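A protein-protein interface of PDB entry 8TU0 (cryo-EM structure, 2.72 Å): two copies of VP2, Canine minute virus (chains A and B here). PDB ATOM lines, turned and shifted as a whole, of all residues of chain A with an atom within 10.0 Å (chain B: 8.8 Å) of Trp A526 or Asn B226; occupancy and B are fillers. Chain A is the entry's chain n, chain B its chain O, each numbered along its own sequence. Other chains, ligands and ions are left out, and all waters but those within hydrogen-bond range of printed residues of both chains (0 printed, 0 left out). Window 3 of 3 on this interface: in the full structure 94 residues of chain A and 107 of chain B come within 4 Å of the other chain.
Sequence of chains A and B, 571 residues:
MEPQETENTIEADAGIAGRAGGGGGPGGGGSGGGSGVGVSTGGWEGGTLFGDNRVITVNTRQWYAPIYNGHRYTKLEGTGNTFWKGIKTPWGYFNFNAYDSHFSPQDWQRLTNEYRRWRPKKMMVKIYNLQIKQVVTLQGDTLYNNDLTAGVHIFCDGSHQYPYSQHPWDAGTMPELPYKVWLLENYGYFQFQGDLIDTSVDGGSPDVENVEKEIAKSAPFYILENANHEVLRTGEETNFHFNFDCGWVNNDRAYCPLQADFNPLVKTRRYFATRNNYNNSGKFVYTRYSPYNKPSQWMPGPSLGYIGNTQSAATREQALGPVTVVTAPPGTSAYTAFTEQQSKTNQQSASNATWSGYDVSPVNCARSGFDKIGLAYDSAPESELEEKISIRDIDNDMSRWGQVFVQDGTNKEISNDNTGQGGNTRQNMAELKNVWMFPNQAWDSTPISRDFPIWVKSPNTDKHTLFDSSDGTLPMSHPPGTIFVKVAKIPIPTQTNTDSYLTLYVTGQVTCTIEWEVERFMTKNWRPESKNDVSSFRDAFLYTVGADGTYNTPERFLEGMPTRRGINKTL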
ATOM      1  N   MET A 522      -3.829 -22.382  16.917  1.00  0.00           N
ATOM      2  CA  MET A 522      -4.956 -22.980  16.229  1.00  0.00           C
ATOM      3  C   MET A 522      -5.945 -23.424  17.289  1.00  0.00           C
ATOM      4  O   MET A 522      -5.540 -23.929  18.338  1.00  0.00           O
ATOM      5  CB  MET A 522      -4.526 -24.172  15.379  1.00  0.00           C
ATOM      6  CG  MET A 522      -3.635 -23.816  14.220  1.00  0.00           C
ATOM      7  SD  MET A 522      -3.037 -25.281  13.359  1.00  0.00           S
ATOM      8  CE  MET A 522      -4.548 -25.867  12.602  1.00  0.00           C
ATOM      9  N   THR A 523      -7.233 -23.226  17.034  1.00  0.00           N
ATOM     10  CA  THR A 523      -8.215 -23.605  18.033  1.00  0.00           C
ATOM     11  C   THR A 523      -9.543 -23.953  17.385  1.00  0.00           C
ATOM     12  O   THR A 523      -9.885 -23.450  16.314  1.00  0.00           O
ATOM     13  CB  THR A 523      -8.419 -22.498  19.057  1.00  0.00           C
ATOM     14  OG1 THR A 523      -9.325 -22.951  20.067  1.00  0.00           O
ATOM     15  CG2 THR A 523      -8.979 -21.294  18.392  1.00  0.00           C
ATOM     16  N   LYS A 524     -10.275 -24.841  18.047  1.00  0.00           N
ATOM     17  CA  LYS A 524     -11.651 -25.136  17.697  1.00  0.00           C
ATOM     18  C   LYS A 524     -12.638 -24.355  18.548  1.00  0.00           C
ATOM     19  O   LYS A 524     -13.844 -24.579  18.438  1.00  0.00           O
ATOM     20  CB  LYS A 524     -11.923 -26.629  17.827  1.00  0.00           C
ATOM     21  CG  LYS A 524     -10.968 -27.488  17.046  1.00  0.00           C
ATOM     22  CD  LYS A 524     -10.906 -27.094  15.593  1.00  0.00           C
ATOM     23  CE  LYS A 524     -12.122 -27.536  14.834  1.00  0.00           C
ATOM     24  NZ  LYS A 524     -11.954 -27.235  13.395  1.00  0.00           N
ATOM     25  N   ASN A 525     -12.150 -23.470  19.410  1.00  0.00           N
ATOM     26  CA  ASN A 525     -13.029 -22.627  20.199  1.00  0.00           C
ATOM     27  C   ASN A 525     -13.955 -21.827  19.303  1.00  0.00           C
ATOM     28  O   ASN A 525     -13.544 -21.305  18.266  1.00  0.00           O
ATOM     29  CB  ASN A 525     -12.214 -21.680  21.063  1.00  0.00           C
ATOM     30  CG  ASN A 525     -13.072 -20.874  21.985  1.00  0.00           C
ATOM     31  OD1 ASN A 525     -14.135 -21.320  22.398  1.00  0.00           O
ATOM     32  ND2 ASN A 525     -12.627 -19.673  22.307  1.00  0.00           N
ATOM     33  N   TRP A 526     -15.221 -21.755  19.696  1.00  0.00           N
ATOM     34  CA  TRP A 526     -16.198 -21.016  18.911  1.00  0.00           C
ATOM     35  C   TRP A 526     -16.170 -19.529  19.232  1.00  0.00           C
ATOM     36  O   TRP A 526     -16.194 -18.698  18.323  1.00  0.00           O
ATOM     37  CB  TRP A 526     -17.586 -21.591  19.164  1.00  0.00           C
ATOM     38  CG  TRP A 526     -18.648 -21.018  18.338  1.00  0.00           C
ATOM     39  CD1 TRP A 526     -19.572 -20.102  18.710  1.00  0.00           C
ATOM     40  CD2 TRP A 526     -18.931 -21.354  16.988  1.00  0.00           C
ATOM     41  NE1 TRP A 526     -20.410 -19.828  17.664  1.00  0.00           N
ATOM     42  CE2 TRP A 526     -20.035 -20.592  16.594  1.00  0.00           C
ATOM     43  CE3 TRP A 526     -18.351 -22.223  16.068  1.00  0.00           C
ATOM     44  CZ2 TRP A 526     -20.560 -20.664  15.325  1.00  0.00           C
ATOM     45  CZ3 TRP A 526     -18.875 -22.296  14.820  1.00  0.00           C
ATOM     46  CH2 TRP A 526     -19.966 -21.522  14.452  1.00  0.00           C
ATOM     47  N   ARG A 527     -16.092 -19.181  20.499  1.00  0.00           N
ATOM     48  CA  ARG A 527     -16.284 -17.821  20.967  1.00  0.00           C
ATOM     49  C   ARG A 527     -15.035 -16.971  20.711  1.00  0.00           C
ATOM     50  O   ARG A 527     -13.930 -17.502  20.597  1.00  0.00           O
ATOM     51  CB  ARG A 527     -16.620 -17.835  22.456  1.00  0.00           C
ATOM     52  CG  ARG A 527     -16.881 -16.463  23.023  1.00  0.00           C
ATOM     53  CD  ARG A 527     -17.060 -16.390  24.502  1.00  0.00           C
ATOM     54  NE  ARG A 527     -18.315 -16.936  24.962  1.00  0.00           N
ATOM     55  CZ  ARG A 527     -18.683 -16.900  26.229  1.00  0.00           C
ATOM     56  NH1 ARG A 527     -19.840 -17.406  26.596  1.00  0.00           N
ATOM     57  NH2 ARG A 527     -17.898 -16.332  27.126  1.00  0.00           N
ATOM     58  N   PRO A 528     -15.183 -15.652  20.581  1.00  0.00           N
ATOM     59  CA  PRO A 528     -14.010 -14.794  20.400  1.00  0.00           C
ATOM     60  C   PRO A 528     -13.171 -14.645  21.663  1.00  0.00           C
ATOM     61  O   PRO A 528     -13.693 -14.570  22.775  1.00  0.00           O
ATOM     62  CB  PRO A 528     -14.626 -13.457  19.991  1.00  0.00           C
ATOM     63  CG  PRO A 528     -15.887 -13.808  19.387  1.00  0.00           C
ATOM     64  CD  PRO A 528     -16.407 -14.951  20.170  1.00  0.00           C
ATOM     65  N   GLU A 529     -11.853 -14.638  21.471  1.00  0.00           N
ATOM     66  CA  GLU A 529     -10.828 -14.464  22.494  1.00  0.00           C
ATOM     67  C   GLU A 529     -10.515 -12.994  22.786  1.00  0.00           C
ATOM     68  O   GLU A 529     -10.759 -12.105  21.971  1.00  0.00           O
ATOM     69  CB  GLU A 529      -9.567 -15.206  22.076  1.00  0.00           C
ATOM     70  CG  GLU A 529      -9.807 -16.693  21.969  1.00  0.00           C
ATOM     71  CD  GLU A 529      -8.587 -17.466  21.536  1.00  0.00           C
ATOM     72  OE1 GLU A 529      -7.573 -16.831  21.176  1.00  0.00           O
ATOM     73  OE2 GLU A 529      -8.650 -18.714  21.546  1.00  0.00           O
ATOM     74  N   ASN A 568      -6.946 -19.598  24.347  1.00  0.00           N
ATOM     75  CA  ASN A 568      -7.371 -20.640  25.260  1.00  0.00           C
ATOM     76  C   ASN A 568      -6.604 -21.922  25.006  1.00  0.00           C
ATOM     77  O   ASN A 568      -6.267 -22.258  23.870  1.00  0.00           O
ATOM     78  CB  ASN A 568      -8.868 -20.890  25.142  1.00  0.00           C
ATOM     79  CG  ASN A 568      -9.674 -19.785  25.751  1.00  0.00           C
ATOM     80  OD1 ASN A 568      -9.793 -19.692  26.970  1.00  0.00           O
ATOM     81  ND2 ASN A 568     -10.227 -18.926  24.912  1.00  0.00           N
ATOM     82  N   THR A 570      -6.684 -25.939  25.906  1.00  0.00           N
ATOM     83  CA  THR A 570      -7.412 -27.066  26.463  1.00  0.00           C
ATOM     84  C   THR A 570      -6.534 -27.801  27.460  1.00  0.00           C
ATOM     85  O   THR A 570      -5.405 -28.191  27.152  1.00  0.00           O
ATOM     86  CB  THR A 570      -7.884 -28.004  25.357  1.00  0.00           C
ATOM     87  OG1 THR A 570      -6.774 -28.375  24.533  1.00  0.00           O
ATOM     88  CG2 THR A 570      -8.942 -27.332  24.518  1.00  0.00           C
ATOM     89  N   TYR B  73     -26.758 -28.468  22.339  1.00  0.00           N
ATOM     90  CA  TYR B  73     -25.845 -28.027  23.375  1.00  0.00           C
ATOM     91  C   TYR B  73     -26.609 -27.186  24.379  1.00  0.00           C
ATOM     92  O   TYR B  73     -27.304 -26.243  24.002  1.00  0.00           O
ATOM     93  CB  TYR B  73     -24.718 -27.207  22.764  1.00  0.00           C
ATOM     94  CG  TYR B  73     -23.794 -27.986  21.876  1.00  0.00           C
ATOM     95  CD1 TYR B  73     -22.597 -28.473  22.350  1.00  0.00           C
ATOM     96  CD2 TYR B  73     -24.131 -28.259  20.574  1.00  0.00           C
ATOM     97  CE1 TYR B  73     -21.754 -29.176  21.541  1.00  0.00           C
ATOM     98  CE2 TYR B  73     -23.300 -28.966  19.765  1.00  0.00           C
ATOM     99  CZ  TYR B  73     -22.115 -29.423  20.250  1.00  0.00           C
ATOM    100  OH  TYR B  73     -21.285 -30.135  19.426  1.00  0.00           O
ATOM    101  N   TRP B  91     -23.481 -35.599  22.188  1.00  0.00           N
ATOM    102  CA  TRP B  91     -22.449 -36.507  21.725  1.00  0.00           C
ATOM    103  C   TRP B  91     -22.163 -37.522  22.814  1.00  0.00           C
ATOM    104  O   TRP B  91     -22.425 -37.287  23.991  1.00  0.00           O
ATOM    105  CB  TRP B  91     -21.158 -35.765  21.366  1.00  0.00           C
ATOM    106  CG  TRP B  91     -21.170 -35.011  20.088  1.00  0.00           C
ATOM    107  CD1 TRP B  91     -21.596 -33.744  19.889  1.00  0.00           C
ATOM    108  CD2 TRP B  91     -20.650 -35.453  18.837  1.00  0.00           C
ATOM    109  NE1 TRP B  91     -21.420 -33.376  18.586  1.00  0.00           N
ATOM    110  CE2 TRP B  91     -20.835 -34.414  17.919  1.00  0.00           C
ATOM    111  CE3 TRP B  91     -20.065 -36.637  18.398  1.00  0.00           C
ATOM    112  CZ2 TRP B  91     -20.456 -34.521  16.595  1.00  0.00           C
ATOM    113  CZ3 TRP B  91     -19.688 -36.735  17.080  1.00  0.00           C
ATOM    114  CH2 TRP B  91     -19.886 -35.689  16.198  1.00  0.00           C
ATOM    115  N   PHE B 155     -16.096 -39.314  15.458  1.00  0.00           N
ATOM    116  CA  PHE B 155     -15.014 -38.349  15.451  1.00  0.00           C
ATOM    117  C   PHE B 155     -14.000 -38.732  16.512  1.00  0.00           C
ATOM    118  O   PHE B 155     -14.334 -38.766  17.698  1.00  0.00           O
ATOM    119  CB  PHE B 155     -15.569 -36.947  15.693  1.00  0.00           C
ATOM    120  CG  PHE B 155     -14.530 -35.930  15.967  1.00  0.00           C
ATOM    121  CD1 PHE B 155     -13.653 -35.545  14.986  1.00  0.00           C
ATOM    122  CD2 PHE B 155     -14.464 -35.318  17.194  1.00  0.00           C
ATOM    123  CE1 PHE B 155     -12.700 -34.615  15.238  1.00  0.00           C
ATOM    124  CE2 PHE B 155     -13.517 -34.377  17.448  1.00  0.00           C
ATOM    125  CZ  PHE B 155     -12.636 -34.023  16.470  1.00  0.00           C
ATOM    126  N   GLN B 161      -8.003 -31.200  20.411  1.00  0.00           N
ATOM    127  CA  GLN B 161      -8.468 -29.842  20.191  1.00  0.00           C
ATOM    128  C   GLN B 161      -9.751 -29.543  20.938  1.00  0.00           C
ATOM    129  O   GLN B 161     -10.120 -28.373  21.056  1.00  0.00           O
ATOM    130  CB  GLN B 161      -8.677 -29.605  18.705  1.00  0.00           C
ATOM    131  CG  GLN B 161      -7.414 -29.631  17.898  1.00  0.00           C
ATOM    132  CD  GLN B 161      -7.693 -29.522  16.425  1.00  0.00           C
ATOM    133  OE1 GLN B 161      -8.771 -29.889  15.963  1.00  0.00           O
ATOM    134  NE2 GLN B 161      -6.730 -29.013  15.676  1.00  0.00           N
ATOM    135  N   TYR B 162     -10.424 -30.552  21.435  1.00  0.00           N
ATOM    136  CA  TYR B 162     -11.622 -30.373  22.217  1.00  0.00           C
ATOM    137  C   TYR B 162     -11.363 -30.787  23.653  1.00  0.00           C
ATOM    138  O   TYR B 162     -10.497 -31.626  23.906  1.00  0.00           O
ATOM    139  CB  TYR B 162     -12.779 -31.193  21.645  1.00  0.00           C
ATOM    140  CG  TYR B 162     -13.252 -30.667  20.324  1.00  0.00           C
ATOM    141  CD1 TYR B 162     -14.149 -29.625  20.268  1.00  0.00           C
ATOM    142  CD2 TYR B 162     -12.803 -31.203  19.139  1.00  0.00           C
ATOM    143  CE1 TYR B 162     -14.578 -29.132  19.082  1.00  0.00           C
ATOM    144  CE2 TYR B 162     -13.230 -30.713  17.942  1.00  0.00           C
ATOM    145  CZ  TYR B 162     -14.118 -29.677  17.920  1.00  0.00           C
ATOM    146  OH  TYR B 162     -14.562 -29.179  16.722  1.00  0.00           O
ATOM    147  N   TYR B 189     -18.408 -30.748  29.129  1.00  0.00           N
ATOM    148  CA  TYR B 189     -17.126 -30.191  29.515  1.00  0.00           C
ATOM    149  C   TYR B 189     -17.305 -28.929  30.337  1.00  0.00           C
ATOM    150  O   TYR B 189     -18.287 -28.202  30.190  1.00  0.00           O
ATOM    151  CB  TYR B 189     -16.265 -29.910  28.287  1.00  0.00           C
ATOM    152  CG  TYR B 189     -16.906 -29.012  27.271  1.00  0.00           C
ATOM    153  CD1 TYR B 189     -16.802 -27.642  27.368  1.00  0.00           C
ATOM    154  CD2 TYR B 189     -17.591 -29.536  26.202  1.00  0.00           C
ATOM    155  CE1 TYR B 189     -17.378 -26.824  26.440  1.00  0.00           C
ATOM    156  CE2 TYR B 189     -18.166 -28.729  25.274  1.00  0.00           C
ATOM    157  CZ  TYR B 189     -18.057 -27.372  25.395  1.00  0.00           C
ATOM    158  OH  TYR B 189     -18.630 -26.552  24.457  1.00  0.00           O
ATOM    159  N   GLN B 191     -16.841 -25.173  31.582  1.00  0.00           N
ATOM    160  CA  GLN B 191     -16.753 -23.923  30.837  1.00  0.00           C
ATOM    161  C   GLN B 191     -16.270 -22.787  31.724  1.00  0.00           C
ATOM    162  O   GLN B 191     -15.179 -22.263  31.497  1.00  0.00           O
ATOM    163  CB  GLN B 191     -18.089 -23.580  30.198  1.00  0.00           C
ATOM    164  CG  GLN B 191     -17.929 -22.515  29.172  1.00  0.00           C
ATOM    165  CD  GLN B 191     -19.185 -22.248  28.418  1.00  0.00           C
ATOM    166  OE1 GLN B 191     -20.219 -22.846  28.684  1.00  0.00           O
ATOM    167  NE2 GLN B 191     -19.100 -21.366  27.437  1.00  0.00           N
ATOM    168  N   ALA B 219     -14.108 -17.195  28.528  1.00  0.00           N
ATOM    169  CA  ALA B 219     -14.366 -18.618  28.640  1.00  0.00           C
ATOM    170  C   ALA B 219     -14.704 -19.195  27.270  1.00  0.00           C
ATOM    171  O   ALA B 219     -15.452 -18.584  26.506  1.00  0.00           O
ATOM    172  CB  ALA B 219     -15.509 -18.886  29.609  1.00  0.00           C
ATOM    173  N   PRO B 220     -14.169 -20.359  26.931  1.00  0.00           N
ATOM    174  CA  PRO B 220     -14.411 -20.943  25.614  1.00  0.00           C
ATOM    175  C   PRO B 220     -15.776 -21.601  25.524  1.00  0.00           C
ATOM    176  O   PRO B 220     -16.438 -21.876  26.520  1.00  0.00           O
ATOM    177  CB  PRO B 220     -13.311 -21.991  25.501  1.00  0.00           C
ATOM    178  CG  PRO B 220     -13.155 -22.446  26.875  1.00  0.00           C
ATOM    179  CD  PRO B 220     -13.362 -21.255  27.765  1.00  0.00           C
ATOM    180  N   PHE B 221     -16.188 -21.841  24.286  1.00  0.00           N
ATOM    181  CA  PHE B 221     -17.331 -22.688  23.991  1.00  0.00           C
ATOM    182  C   PHE B 221     -16.982 -23.531  22.783  1.00  0.00           C
ATOM    183  O   PHE B 221     -16.649 -22.986  21.730  1.00  0.00           O
ATOM    184  CB  PHE B 221     -18.581 -21.852  23.741  1.00  0.00           C
ATOM    185  CG  PHE B 221     -19.721 -22.622  23.167  1.00  0.00           C
ATOM    186  CD1 PHE B 221     -20.415 -23.524  23.927  1.00  0.00           C
ATOM    187  CD2 PHE B 221     -20.130 -22.395  21.880  1.00  0.00           C
ATOM    188  CE1 PHE B 221     -21.461 -24.214  23.397  1.00  0.00           C
ATOM    189  CE2 PHE B 221     -21.181 -23.078  21.359  1.00  0.00           C
ATOM    190  CZ  PHE B 221     -21.845 -23.991  22.115  1.00  0.00           C
ATOM    191  N   TYR B 222     -17.052 -24.846  22.930  1.00  0.00           N
ATOM    192  CA  TYR B 222     -16.629 -25.766  21.890  1.00  0.00           C
ATOM    193  C   TYR B 222     -17.821 -26.488  21.286  1.00  0.00           C
ATOM    194  O   TYR B 222     -18.758 -26.866  21.992  1.00  0.00           O
ATOM    195  CB  TYR B 222     -15.643 -26.791  22.431  1.00  0.00           C
ATOM    196  CG  TYR B 222     -14.349 -26.191  22.877  1.00  0.00           C
ATOM    197  CD1 TYR B 222     -13.331 -25.972  21.980  1.00  0.00           C
ATOM    198  CD2 TYR B 222     -14.144 -25.850  24.193  1.00  0.00           C
ATOM    199  CE1 TYR B 222     -12.152 -25.428  22.381  1.00  0.00           C
ATOM    200  CE2 TYR B 222     -12.968 -25.308  24.603  1.00  0.00           C
ATOM    201  CZ  TYR B 222     -11.972 -25.095  23.692  1.00  0.00           C
ATOM    202  OH  TYR B 222     -10.783 -24.546  24.092  1.00  0.00           O
ATOM    203  N   ILE B 223     -17.756 -26.684  19.979  1.00  0.00           N
ATOM    204  CA  ILE B 223     -18.761 -27.389  19.200  1.00  0.00           C
ATOM    205  C   ILE B 223     -18.053 -28.439  18.364  1.00  0.00           C
ATOM    206  O   ILE B 223     -17.083 -28.126  17.668  1.00  0.00           O
ATOM    207  CB  ILE B 223     -19.544 -26.420  18.300  1.00  0.00           C
ATOM    208  CG1 ILE B 223     -20.541 -25.624  19.122  1.00  0.00           C
ATOM    209  CG2 ILE B 223     -20.188 -27.130  17.152  1.00  0.00           C
ATOM    210  CD1 ILE B 223     -21.254 -24.597  18.317  1.00  0.00           C
ATOM    211  N   LEU B 224     -18.530 -29.674  18.419  1.00  0.00           N
ATOM    212  CA  LEU B 224     -17.837 -30.731  17.700  1.00  0.00           C
ATOM    213  C   LEU B 224     -18.206 -30.796  16.231  1.00  0.00           C
ATOM    214  O   LEU B 224     -17.682 -31.660  15.524  1.00  0.00           O
ATOM    215  CB  LEU B 224     -18.096 -32.093  18.338  1.00  0.00           C
ATOM    216  CG  LEU B 224     -17.214 -32.507  19.508  1.00  0.00           C
ATOM    217  CD1 LEU B 224     -17.538 -31.712  20.744  1.00  0.00           C
ATOM    218  CD2 LEU B 224     -17.364 -33.962  19.772  1.00  0.00           C
ATOM    219  N   GLU B 225     -19.092 -29.935  15.756  1.00  0.00           N
ATOM    220  CA  GLU B 225     -19.404 -29.880  14.338  1.00  0.00           C
ATOM    221  C   GLU B 225     -18.449 -29.004  13.549  1.00  0.00           C
ATOM    222  O   GLU B 225     -18.585 -28.915  12.329  1.00  0.00           O
ATOM    223  CB  GLU B 225     -20.835 -29.404  14.122  1.00  0.00           C
ATOM    224  CG  GLU B 225     -21.890 -30.441  14.425  1.00  0.00           C
ATOM    225  CD  GLU B 225     -22.285 -30.503  15.877  1.00  0.00           C
ATOM    226  OE1 GLU B 225     -21.683 -29.791  16.699  1.00  0.00           O
ATOM    227  OE2 GLU B 225     -23.216 -31.269  16.192  1.00  0.00           O
ATOM    228  N   ASN B 226     -17.493 -28.351  14.199  1.00  0.00           N
ATOM    229  CA  ASN B 226     -16.448 -27.667  13.456  1.00  0.00           C
ATOM    230  C   ASN B 226     -15.437 -28.630  12.876  1.00  0.00           C
ATOM    231  O   ASN B 226     -14.703 -28.262  11.958  1.00  0.00           O
ATOM    232  CB  ASN B 226     -15.708 -26.687  14.349  1.00  0.00           C
ATOM    233  CG  ASN B 226     -16.526 -25.487  14.687  1.00  0.00           C
ATOM    234  OD1 ASN B 226     -17.444 -25.133  13.958  1.00  0.00           O
ATOM    235  ND2 ASN B 226     -16.195 -24.838  15.795  1.00  0.00           N
ATOM    236  N   ALA B 227     -15.372 -29.843  13.387  1.00  0.00           N
ATOM    237  CA  ALA B 227     -14.265 -30.737  13.106  1.00  0.00           C
ATOM    238  C   ALA B 227     -14.619 -31.683  11.972  1.00  0.00           C
ATOM    239  O   ALA B 227     -15.765 -32.110  11.837  1.00  0.00           O
ATOM    240  CB  ALA B 227     -13.894 -31.526  14.356  1.00  0.00           C
ATOM    241  N   ASN B 228     -13.627 -31.985  11.147  1.00  0.00           N
ATOM    242  CA  ASN B 228     -13.799 -32.991  10.118  1.00  0.00           C
ATOM    243  C   ASN B 228     -14.009 -34.339  10.779  1.00  0.00           C
ATOM    244  O   ASN B 228     -13.212 -34.750  11.624  1.00  0.00           O
ATOM    245  CB  ASN B 228     -12.569 -33.038   9.226  1.00  0.00           C
ATOM    246  CG  ASN B 228     -12.367 -31.769   8.461  1.00  0.00           C
ATOM    247  OD1 ASN B 228     -12.978 -31.551   7.422  1.00  0.00           O
ATOM    248  ND2 ASN B 228     -11.524 -30.901   8.986  1.00  0.00           N
ATOM    249  N   HIS B 229     -15.074 -35.030  10.403  1.00  0.00           N
ATOM    250  CA  HIS B 229     -15.289 -36.356  10.947  1.00  0.00           C
ATOM    251  C   HIS B 229     -16.175 -37.144  10.004  1.00  0.00           C
ATOM    252  O   HIS B 229     -16.807 -36.588   9.107  1.00  0.00           O
ATOM    253  CB  HIS B 229     -15.883 -36.296  12.349  1.00  0.00           C
ATOM    254  CG  HIS B 229     -17.205 -35.611  12.426  1.00  0.00           C
ATOM    255  ND1 HIS B 229     -18.384 -36.231  12.085  1.00  0.00           N
ATOM    256  CD2 HIS B 229     -17.539 -34.368  12.837  1.00  0.00           C
ATOM    257  CE1 HIS B 229     -19.388 -35.396  12.275  1.00  0.00           C
ATOM    258  NE2 HIS B 229     -18.902 -34.256  12.725  1.00  0.00           N
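The backbone NH (N) of Phe B221 is in hydrogen-bond range of the side-chain amide oxygen (OD1) of Asn A525 (2.8 Å).
O of Asn B226 is in hydrogen-bond range of NZ of Lys A524 (3.3 Å).
The backbone NH (N) of Trp A526 sits at hydrogen-bond distance from the backbone carbonyl oxygen (O) of Phe B221, at 2.8 Å.
O of Ala B219 lies close to NH2 of Arg A527 (3.4 Å).
OH of Tyr B162 sits close to N of Ala B227, 3.5 Å away.
ND2 of Asn A525 is in hydrogen-bond range of O of Arg A527.
The side-chain amide nitrogen (NE2) of Gln B191 is in hydrogen-bond range of the backbone carbonyl oxygen (O) of Pro B220 (2.9 Å).
The backbone NH of Asn A568 is in hydrogen-bond range of the side-chain carboxylate of Glu A529.
O of Ile B223 sits at hydrogen-bond distance from OH of Tyr B162, 2.9 Å away.
The side-chain hydroxyl (OH) of Tyr B189 lies within hydrogen-bond range of the backbone carbonyl oxygen (O) of Tyr B222 (2.5 Å).
Among the printed residues, merely in contact across the chains: Asn A525 with Pro B220 (3.2 Å), Trp A526 with Asn B226 (3.3 Å), Thr A570 with Tyr B222 (3.4 Å), Lys A524 with Gln B161 (3.4 Å), Lys A524 with Tyr B162 (3.5 Å), Asn A525 with Tyr B222 (3.6 Å), Thr A570 with Gln B161 (3.8 Å), Lys A524 with Tyr B222 (3.8 Å) and Asn A568 with Pro B220 (3.98 Å).
Of the printed residues of chain B, Asn A525 touches Pro B220 (3.2 Å), Phe B221 (2.8 Å) and Tyr B222 (3.6 Å).
Trp A526 touches just these residues of chain B: Phe B221 and Asn B226.
Printed residues of chain B within 4 Å of Arg A527: Ala B219.
Of the printed residues of chain A, Tyr B222 touches Lys A524, Asn A525 and Thr A570.
Asn B226 touches just these residues of chain A: Lys A524 (3.3 Å) and Trp A526 (3.3 Å).
No residue of chain A comes within 4 Å of Ala B227.
The nearest residue of chain A that does not touch Asn B226 is Asn A525 (5.1 Å).
Of the 18 printed residues of chain B, 7 touch a printed residue of chain A.
Hydrophobic or aromatic side chains of chain B that line the printed part of chain A: Tyr B162, Pro B220, Phe B221 and Tyr B222.
No position is printed for both chains.
Of the 13 pairs that touch across the chains among the printed residues, none has its exchanged pair printed and touching as well.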
